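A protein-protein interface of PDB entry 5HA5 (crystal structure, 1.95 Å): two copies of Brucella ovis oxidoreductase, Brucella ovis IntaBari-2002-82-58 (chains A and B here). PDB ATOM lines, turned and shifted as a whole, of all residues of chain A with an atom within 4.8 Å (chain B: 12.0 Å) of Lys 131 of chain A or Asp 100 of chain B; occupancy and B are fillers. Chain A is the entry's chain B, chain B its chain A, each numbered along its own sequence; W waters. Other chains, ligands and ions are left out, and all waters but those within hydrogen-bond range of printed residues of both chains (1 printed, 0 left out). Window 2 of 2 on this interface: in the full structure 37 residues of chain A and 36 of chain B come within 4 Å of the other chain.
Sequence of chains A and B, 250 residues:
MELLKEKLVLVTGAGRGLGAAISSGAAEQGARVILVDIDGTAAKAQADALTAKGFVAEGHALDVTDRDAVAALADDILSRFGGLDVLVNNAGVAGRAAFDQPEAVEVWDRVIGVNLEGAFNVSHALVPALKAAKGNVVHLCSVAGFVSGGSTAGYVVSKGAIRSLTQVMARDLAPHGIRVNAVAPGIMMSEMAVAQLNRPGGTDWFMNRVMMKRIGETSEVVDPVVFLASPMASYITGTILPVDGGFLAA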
ATOM      1  N   HIS A 124      -9.079  18.005  15.253  1.00  0.00           N
ATOM      2  CA  HIS A 124      -8.133  17.569  14.234  1.00  0.00           C
ATOM      3  C   HIS A 124      -8.740  17.686  12.838  1.00  0.00           C
ATOM      4  O   HIS A 124      -8.082  18.163  11.902  1.00  0.00           O
ATOM      5  CB  HIS A 124      -7.673  16.133  14.519  1.00  0.00           C
ATOM      6  CG  HIS A 124      -6.620  15.653  13.570  1.00  0.00           C
ATOM      7  ND1 HIS A 124      -6.916  15.052  12.362  1.00  0.00           N
ATOM      8  CD2 HIS A 124      -5.270  15.729  13.634  1.00  0.00           C
ATOM      9  CE1 HIS A 124      -5.792  14.771  11.730  1.00  0.00           C
ATOM     10  NE2 HIS A 124      -4.779  15.170  12.479  1.00  0.00           N
ATOM     11  N   VAL A 127      -8.876  21.324  11.182  1.00  0.00           N
ATOM     12  CA  VAL A 127      -7.656  22.114  11.018  1.00  0.00           C
ATOM     13  C   VAL A 127      -7.531  22.707   9.617  1.00  0.00           C
ATOM     14  O   VAL A 127      -7.239  23.910   9.506  1.00  0.00           O
ATOM     15  CB  VAL A 127      -6.426  21.268  11.411  1.00  0.00           C
ATOM     16  CG1 VAL A 127      -5.145  21.930  10.888  1.00  0.00           C
ATOM     17  CG2 VAL A 127      -6.367  21.058  12.945  1.00  0.00           C
ATOM     18  N   PRO A 128      -7.710  21.953   8.526  1.00  0.00           N
ATOM     19  CA  PRO A 128      -7.644  22.602   7.202  1.00  0.00           C
ATOM     20  C   PRO A 128      -8.573  23.800   7.089  1.00  0.00           C
ATOM     21  O   PRO A 128      -8.159  24.857   6.594  1.00  0.00           O
ATOM     22  CB  PRO A 128      -8.026  21.469   6.239  1.00  0.00           C
ATOM     23  CG  PRO A 128      -7.557  20.231   6.928  1.00  0.00           C
ATOM     24  CD  PRO A 128      -7.840  20.489   8.399  1.00  0.00           C
ATOM     25  N   ALA A 129      -9.817  23.676   7.552  1.00  0.00           N
ATOM     26  CA  ALA A 129     -10.740  24.806   7.458  1.00  0.00           C
ATOM     27  C   ALA A 129     -10.306  25.958   8.361  1.00  0.00           C
ATOM     28  O   ALA A 129     -10.417  27.130   7.982  1.00  0.00           O
ATOM     29  CB  ALA A 129     -12.164  24.356   7.793  1.00  0.00           C
ATOM     30  N   LEU A 130      -9.802  25.649   9.556  1.00  0.00           N
ATOM     31  CA  LEU A 130      -9.343  26.713  10.448  1.00  0.00           C
ATOM     32  C   LEU A 130      -8.120  27.423   9.879  1.00  0.00           C
ATOM     33  O   LEU A 130      -7.971  28.644  10.037  1.00  0.00           O
ATOM     34  CB  LEU A 130      -9.021  26.133  11.823  1.00  0.00           C
ATOM     35  CG  LEU A 130     -10.226  25.673  12.643  1.00  0.00           C
ATOM     36  CD1 LEU A 130      -9.752  24.783  13.804  1.00  0.00           C
ATOM     37  CD2 LEU A 130     -10.976  26.893  13.155  1.00  0.00           C
ATOM     38  N   LYS A 131      -7.223  26.674   9.233  1.00  0.00           N
ATOM     39  CA  LYS A 131      -6.044  27.284   8.619  1.00  0.00           C
ATOM     40  C   LYS A 131      -6.436  28.257   7.523  1.00  0.00           C
ATOM     41  O   LYS A 131      -5.816  29.319   7.365  1.00  0.00           O
ATOM     42  CB  LYS A 131      -5.135  26.217   8.013  1.00  0.00           C
ATOM     43  CG  LYS A 131      -4.383  25.335   8.996  1.00  0.00           C
ATOM     44  CD  LYS A 131      -3.436  24.394   8.235  1.00  0.00           C
ATOM     45  CE  LYS A 131      -2.470  23.672   9.188  1.00  0.00           C
ATOM     46  NZ  LYS A 131      -1.556  22.710   8.485  1.00  0.00           N
ATOM     47  N   ALA A 132      -7.422  27.878   6.716  1.00  0.00           N
ATOM     48  CA  ALA A 132      -7.792  28.700   5.565  1.00  0.00           C
ATOM     49  C   ALA A 132      -8.342  30.049   6.011  1.00  0.00           C
ATOM     50  O   ALA A 132      -8.085  31.078   5.371  1.00  0.00           O
ATOM     51  CB  ALA A 132      -8.808  27.947   4.711  1.00  0.00           C
ATOM     52  N   ALA A 133      -9.090  30.063   7.115  1.00  0.00           N
ATOM     53  CA  ALA A 133      -9.695  31.271   7.652  1.00  0.00           C
ATOM     54  C   ALA A 133      -8.858  31.930   8.740  1.00  0.00           C
ATOM     55  O   ALA A 133      -9.210  33.022   9.189  1.00  0.00           O
ATOM     56  CB  ALA A 133     -11.087  30.951   8.207  1.00  0.00           C
ATOM     57  N   LYS A 134      -7.745  31.314   9.150  1.00  0.00           N
ATOM     58  CA  LYS A 134      -7.038  31.696  10.372  1.00  0.00           C
ATOM     59  C   LYS A 134      -8.029  31.872  11.520  1.00  0.00           C
ATOM     60  O   LYS A 134      -8.074  32.901  12.201  1.00  0.00           O
ATOM     61  CB  LYS A 134      -6.188  32.947  10.154  1.00  0.00           C
ATOM     62  CG  LYS A 134      -5.093  32.709   9.117  1.00  0.00           C
ATOM     63  CD  LYS A 134      -4.175  33.901   8.953  1.00  0.00           C
ATOM     64  CE  LYS A 134      -2.965  33.511   8.118  1.00  0.00           C
ATOM     65  NZ  LYS A 134      -2.049  34.657   7.909  1.00  0.00           N
ATOM     66  N   LEU A 173      -0.636  24.921  16.240  1.00  0.00           N
ATOM     67  CA  LEU A 173      -1.403  25.706  15.280  1.00  0.00           C
ATOM     68  C   LEU A 173      -1.058  27.198  15.283  1.00  0.00           C
ATOM     69  O   LEU A 173      -1.428  27.902  14.332  1.00  0.00           O
ATOM     70  CB  LEU A 173      -2.906  25.507  15.530  1.00  0.00           C
ATOM     71  CG  LEU A 173      -3.323  24.029  15.505  1.00  0.00           C
ATOM     72  CD1 LEU A 173      -4.811  23.855  15.872  1.00  0.00           C
ATOM     73  CD2 LEU A 173      -3.003  23.407  14.121  1.00  0.00           C
ATOM     74  N   HIS A 176       0.174  28.738  12.111  1.00  0.00           N
ATOM     75  CA  HIS A 176      -0.848  28.893  11.088  1.00  0.00           C
ATOM     76  C   HIS A 176      -1.859  29.979  11.423  1.00  0.00           C
ATOM     77  O   HIS A 176      -2.891  30.072  10.755  1.00  0.00           O
ATOM     78  CB  HIS A 176      -1.544  27.550  10.857  1.00  0.00           C
ATOM     79  CG  HIS A 176      -0.592  26.460  10.481  1.00  0.00           C
ATOM     80  ND1 HIS A 176      -0.083  26.327   9.205  1.00  0.00           N
ATOM     81  CD2 HIS A 176      -0.014  25.486  11.222  1.00  0.00           C
ATOM     82  CE1 HIS A 176       0.765  25.313   9.176  1.00  0.00           C
ATOM     83  NE2 HIS A 176       0.823  24.784  10.388  1.00  0.00           N
ATOM     84  N   ILE A 178      -3.748  30.296  14.157  1.00  0.00           N
ATOM     85  CA  ILE A 178      -4.928  29.747  14.827  1.00  0.00           C
ATOM     86  C   ILE A 178      -4.700  29.810  16.337  1.00  0.00           C
ATOM     87  O   ILE A 178      -3.788  29.162  16.859  1.00  0.00           O
ATOM     88  CB  ILE A 178      -5.198  28.299  14.382  1.00  0.00           C
ATOM     89  CG1 ILE A 178      -5.487  28.222  12.880  1.00  0.00           C
ATOM     90  CG2 ILE A 178      -6.306  27.644  15.250  1.00  0.00           C
ATOM     91  CD1 ILE A 178      -5.382  26.800  12.336  1.00  0.00           C
ATOM     92  N   ARG B  96       6.119  11.055  17.625  1.00  0.00           N
ATOM     93  CA  ARG B  96       6.399  12.305  16.935  1.00  0.00           C
ATOM     94  C   ARG B  96       5.324  12.520  15.883  1.00  0.00           C
ATOM     95  O   ARG B  96       5.165  11.692  14.983  1.00  0.00           O
ATOM     96  CB  ARG B  96       7.787  12.286  16.289  1.00  0.00           C
ATOM     97  N   ALA B  97       4.589  13.625  16.007  1.00  0.00           N
ATOM     98  CA  ALA B  97       3.590  14.044  15.030  1.00  0.00           C
ATOM     99  C   ALA B  97       3.035  15.393  15.459  1.00  0.00           C
ATOM    100  O   ALA B  97       2.656  15.557  16.623  1.00  0.00           O
ATOM    101  CB  ALA B  97       2.449  13.031  14.908  1.00  0.00           C
ATOM    102  N   ALA B  98       3.001  16.363  14.541  1.00  0.00           N
ATOM    103  CA  ALA B  98       2.355  17.637  14.813  1.00  0.00           C
ATOM    104  C   ALA B  98       0.842  17.509  14.653  1.00  0.00           C
ATOM    105  O   ALA B  98       0.342  16.665  13.900  1.00  0.00           O
ATOM    106  CB  ALA B  98       2.900  18.727  13.881  1.00  0.00           C
ATOM    107  N   PHE B  99       0.110  18.381  15.353  1.00  0.00           N
ATOM    108  CA  PHE B  99      -1.348  18.263  15.400  1.00  0.00           C
ATOM    109  C   PHE B  99      -1.977  18.361  14.017  1.00  0.00           C
ATOM    110  O   PHE B  99      -3.010  17.734  13.764  1.00  0.00           O
ATOM    111  CB  PHE B  99      -1.956  19.341  16.301  1.00  0.00           C
ATOM    112  CG  PHE B  99      -3.371  19.058  16.682  1.00  0.00           C
ATOM    113  CD1 PHE B  99      -3.653  18.178  17.724  1.00  0.00           C
ATOM    114  CD2 PHE B  99      -4.427  19.653  15.995  1.00  0.00           C
ATOM    115  CE1 PHE B  99      -4.962  17.887  18.070  1.00  0.00           C
ATOM    116  CE2 PHE B  99      -5.741  19.379  16.340  1.00  0.00           C
ATOM    117  CZ  PHE B  99      -6.011  18.492  17.378  1.00  0.00           C
ATOM    118  N   ASP B 100      -1.384  19.131  13.112  1.00  0.00           N
ATOM    119  CA  ASP B 100      -1.964  19.297  11.782  1.00  0.00           C
ATOM    120  C   ASP B 100      -1.544  18.208  10.803  1.00  0.00           C
ATOM    121  O   ASP B 100      -1.826  18.326   9.604  1.00  0.00           O
ATOM    122  CB  ASP B 100      -1.627  20.683  11.225  1.00  0.00           C
ATOM    123  CG  ASP B 100      -0.130  20.907  11.013  1.00  0.00           C
ATOM    124  OD1 ASP B 100       0.693  20.335  11.752  1.00  0.00           O
ATOM    125  OD2 ASP B 100       0.217  21.709  10.123  1.00  0.00           O
ATOM    126  N   GLN B 101      -0.896  17.181  11.264  1.00  0.00           N
ATOM    127  CA  GLN B 101      -0.558  16.120  10.326  1.00  0.00           C
ATOM    128  C   GLN B 101      -1.550  14.971  10.449  1.00  0.00           C
ATOM    129  O   GLN B 101      -2.041  14.683  11.550  1.00  0.00           O
ATOM    130  CB  GLN B 101       0.849  15.573  10.588  1.00  0.00           C
ATOM    131  CG  GLN B 101       1.982  16.580  10.569  1.00  0.00           C
ATOM    132  CD  GLN B 101       3.344  15.906  10.751  1.00  0.00           C
ATOM    133  OE1 GLN B 101       3.840  15.749  11.876  1.00  0.00           O
ATOM    134  NE2 GLN B 101       3.948  15.489   9.640  1.00  0.00           N
ATOM    135  N   PRO B 102      -1.857  14.284   9.343  1.00  0.00           N
ATOM    136  CA  PRO B 102      -2.709  13.087   9.456  1.00  0.00           C
ATOM    137  C   PRO B 102      -2.135  12.053  10.400  1.00  0.00           C
ATOM    138  O   PRO B 102      -2.896  11.399  11.127  1.00  0.00           O
ATOM    139  CB  PRO B 102      -2.772  12.560   8.013  1.00  0.00           C
ATOM    140  CG  PRO B 102      -2.490  13.749   7.169  1.00  0.00           C
ATOM    141  CD  PRO B 102      -1.500  14.579   7.945  1.00  0.00           C
ATOM    142  N   GLU B 103      -0.802  11.905  10.415  1.00  0.00           N
ATOM    143  CA  GLU B 103      -0.129  10.968  11.313  1.00  0.00           C
ATOM    144  C   GLU B 103      -0.475  11.201  12.779  1.00  0.00           C
ATOM    145  O   GLU B 103      -0.295  10.292  13.605  1.00  0.00           O
ATOM    146  CB  GLU B 103       1.389  11.071  11.135  1.00  0.00           C
ATOM    147  CG  GLU B 103       1.910  10.627   9.775  1.00  0.00           C
ATOM    148  CD  GLU B 103       1.661  11.649   8.663  1.00  0.00           C
ATOM    149  OE1 GLU B 103       1.142  12.750   8.946  1.00  0.00           O
ATOM    150  OE2 GLU B 103       1.988  11.344   7.498  1.00  0.00           O
ATOM    151  N   ALA B 104      -0.943  12.398  13.130  1.00  0.00           N
ATOM    152  CA  ALA B 104      -1.196  12.674  14.539  1.00  0.00           C
ATOM    153  C   ALA B 104      -2.253  11.740  15.104  1.00  0.00           C
ATOM    154  O   ALA B 104      -2.250  11.462  16.304  1.00  0.00           O
ATOM    155  CB  ALA B 104      -1.613  14.135  14.729  1.00  0.00           C
ATOM    156  N   VAL B 105      -3.144  11.224  14.257  1.00  0.00           N
ATOM    157  CA  VAL B 105      -4.246  10.411  14.758  1.00  0.00           C
ATOM    158  C   VAL B 105      -3.737   9.056  15.232  1.00  0.00           C
ATOM    159  O   VAL B 105      -4.047   8.627  16.346  1.00  0.00           O
ATOM    160  CB  VAL B 105      -5.340  10.269  13.686  1.00  0.00           C
ATOM    161  CG1 VAL B 105      -6.411   9.282  14.152  1.00  0.00           C
ATOM    162  CG2 VAL B 105      -5.946  11.632  13.384  1.00  0.00           C
ATOM    163  N   GLU B 106      -2.946   8.360  14.403  1.00  0.00           N
ATOM    164  CA  GLU B 106      -2.433   7.060  14.835  1.00  0.00           C
ATOM    165  C   GLU B 106      -1.546   7.205  16.064  1.00  0.00           C
ATOM    166  O   GLU B 106      -1.593   6.375  16.981  1.00  0.00           O
ATOM    167  CB  GLU B 106      -1.678   6.371  13.690  1.00  0.00           C
ATOM    168  N   VAL B 107      -0.741   8.264  16.115  1.00  0.00           N
ATOM    169  CA  VAL B 107       0.095   8.478  17.292  1.00  0.00           C
ATOM    170  C   VAL B 107      -0.772   8.729  18.523  1.00  0.00           C
ATOM    171  O   VAL B 107      -0.543   8.157  19.596  1.00  0.00           O
ATOM    172  CB  VAL B 107       1.084   9.629  17.042  1.00  0.00           C
ATOM    173  CG1 VAL B 107       1.736  10.037  18.357  1.00  0.00           C
ATOM    174  CG2 VAL B 107       2.145   9.193  16.015  1.00  0.00           C
ATOM    175  N   TRP B 108      -1.784   9.594  18.380  1.00  0.00           N
ATOM    176  CA  TRP B 108      -2.702   9.880  19.476  1.00  0.00           C
ATOM    177  C   TRP B 108      -3.356   8.613  20.019  1.00  0.00           C
ATOM    178  O   TRP B 108      -3.378   8.385  21.233  1.00  0.00           O
ATOM    179  CB  TRP B 108      -3.758  10.871  18.994  1.00  0.00           C
ATOM    180  CG  TRP B 108      -4.892  11.113  19.934  1.00  0.00           C
ATOM    181  CD1 TRP B 108      -5.987  10.319  20.130  1.00  0.00           C
ATOM    182  CD2 TRP B 108      -5.081  12.268  20.747  1.00  0.00           C
ATOM    183  NE1 TRP B 108      -6.840  10.903  21.028  1.00  0.00           N
ATOM    184  CE2 TRP B 108      -6.310  12.102  21.426  1.00  0.00           C
ATOM    185  CE3 TRP B 108      -4.330  13.430  20.968  1.00  0.00           C
ATOM    186  CZ2 TRP B 108      -6.797  13.047  22.337  1.00  0.00           C
ATOM    187  CZ3 TRP B 108      -4.821  14.378  21.843  1.00  0.00           C
ATOM    188  CH2 TRP B 108      -6.042  14.173  22.533  1.00  0.00           C
ATOM    189  N   SER B 151       6.562  17.611  23.146  1.00  0.00           N
ATOM    190  CA  SER B 151       5.984  16.290  22.932  1.00  0.00           C
ATOM    191  C   SER B 151       4.761  16.325  22.011  1.00  0.00           C
ATOM    192  O   SER B 151       4.115  17.356  21.817  1.00  0.00           O
ATOM    193  CB  SER B 151       5.599  15.669  24.275  1.00  0.00           C
ATOM    194  OG  SER B 151       6.704  15.668  25.167  1.00  0.00           O
ATOM    195  N   THR B 152       4.440  15.163  21.451  1.00  0.00           N
ATOM    196  CA  THR B 152       3.297  15.073  20.555  1.00  0.00           C
ATOM    197  C   THR B 152       1.994  15.213  21.344  1.00  0.00           C
ATOM    198  O   THR B 152       1.930  14.931  22.544  1.00  0.00           O
ATOM    199  CB  THR B 152       3.321  13.742  19.784  1.00  0.00           C
ATOM    200  OG1 THR B 152       2.352  13.786  18.732  1.00  0.00           O
ATOM    201  CG2 THR B 152       3.020  12.545  20.746  1.00  0.00           C
ATOM    202  N   ALA B 153       0.949  15.674  20.650  1.00  0.00           N
ATOM    203  CA  ALA B 153      -0.329  15.950  21.303  1.00  0.00           C
ATOM    204  C   ALA B 153      -0.816  14.777  22.154  1.00  0.00           C
ATOM    205  O   ALA B 153      -1.245  14.963  23.298  1.00  0.00           O
ATOM    206  CB  ALA B 153      -1.375  16.324  20.251  1.00  0.00           C
ATOM    207  N   GLY B 154      -0.767  13.555  21.618  1.00  0.00           N
ATOM    208  CA  GLY B 154      -1.239  12.426  22.410  1.00  0.00           C
ATOM    209  C   GLY B 154      -0.481  12.274  23.716  1.00  0.00           C
ATOM    210  O   GLY B 154      -1.059  11.898  24.737  1.00  0.00           O
HETATM  211  O   HOH W   1      -5.115  18.217  11.759  1.00  0.00           O
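The backbone carbonyl oxygen (O) of Phe 99 of chain B lies close to a ring nitrogen (NE2) of His 124 of chain A (3.4 Å). OD2 of Asp 100 of chain B lies within salt-bridge range of NZ of Lys 131 of chain A, 2.6 Å away. A ring nitrogen (NE2) of His 176 of chain A lies within hydrogen-bond range of the side-chain carboxylate (OD2) of Asp 100 of chain B. A ring nitrogen (NE2) of His 124 of chain A is in hydrogen-bond range of the backbone carbonyl oxygen (O) of Gln 101 of chain B.
No position is printed for both chains.
Water W1 lies within hydrogen-bond range of the backbone carbonyl oxygen (O) of Phe 99 of chain B (2.9 Å) and the backbone carbonyl oxygen (O) of His 124 of chain A (3.0 Å).
Among the printed residues, merely in contact across the chains: His 124 of chain A with Val 105 of chain B (3.6 Å), Val 127 of chain A with Phe 99 of chain B (3.8 Å) and Val 127 of chain A with Asp 100 of chain B (3.7 Å).
OE1 of Gln 101 of chain B sits at hydrogen-bond distance from N of Ala 98 of chain B, 2.9 Å away.
Lys 131 of chain A touches just one residue of chain B: Asp 100 (2.6 Å). Asp 100 of chain B touches three residues of chain A. Of chain B, only Phe 99 and Asp 100 come within 4 Å of Val 127 of chain A. No residue of chain B comes within 4 Å of Pro 128 of chain A. Ala 132 of chain A touches none of the printed residues of chain B. No residue of chain B comes within 4 Å of Ala 133 of chain A. No residue of chain B comes within 4 Å of Leu 173 of chain A. His 176 of chain A touches one residue of chain B. Of the printed residues of chain A, Phe 99 of chain B touches His 124 (3.0 Å) and Val 127 (3.8 Å). Printed residues of chain A within 4 Å of Val 105 of chain B: His 124. Of the printed residues of chain A, Gln 101 of chain B touches His 124 (2.9 Å). Of the printed residues of chain B, His 124 of chain A touches Phe 99 (3.0 Å), Gln 101 (2.9 Å) and Val 105 (3.6 Å). The nearest residue of chain B that does not touch Lys 131 of chain A is Gln 101 of chain B (6.2 Å). The nearest residue of chain A that does not touch Asp 100 of chain B is Leu 173 of chain A (4.2 Å).
Hydrophobic or aromatic side chains of chain B that line the printed part of chain A: Phe 99 and Val 105. Of the 12 printed residues of chain A, 4 touch a printed residue of chain B. Printed residues of chain A that touch a printed residue of chain B: His 124, Val 127, Lys 131 and His 176. Hydrophobic or aromatic side chains of chain A that line the printed part of chain B: His 124, Val 127 and His 176. Along chain A the printed residues that touch a printed residue of chain B span positions 124 to 176. Among the printed residues, Asp or Glu carboxylates within 4 Å of a Lys or Arg side-chain nitrogen of the other chain: Lys 131 of chain A with Asp 100 of chain B.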
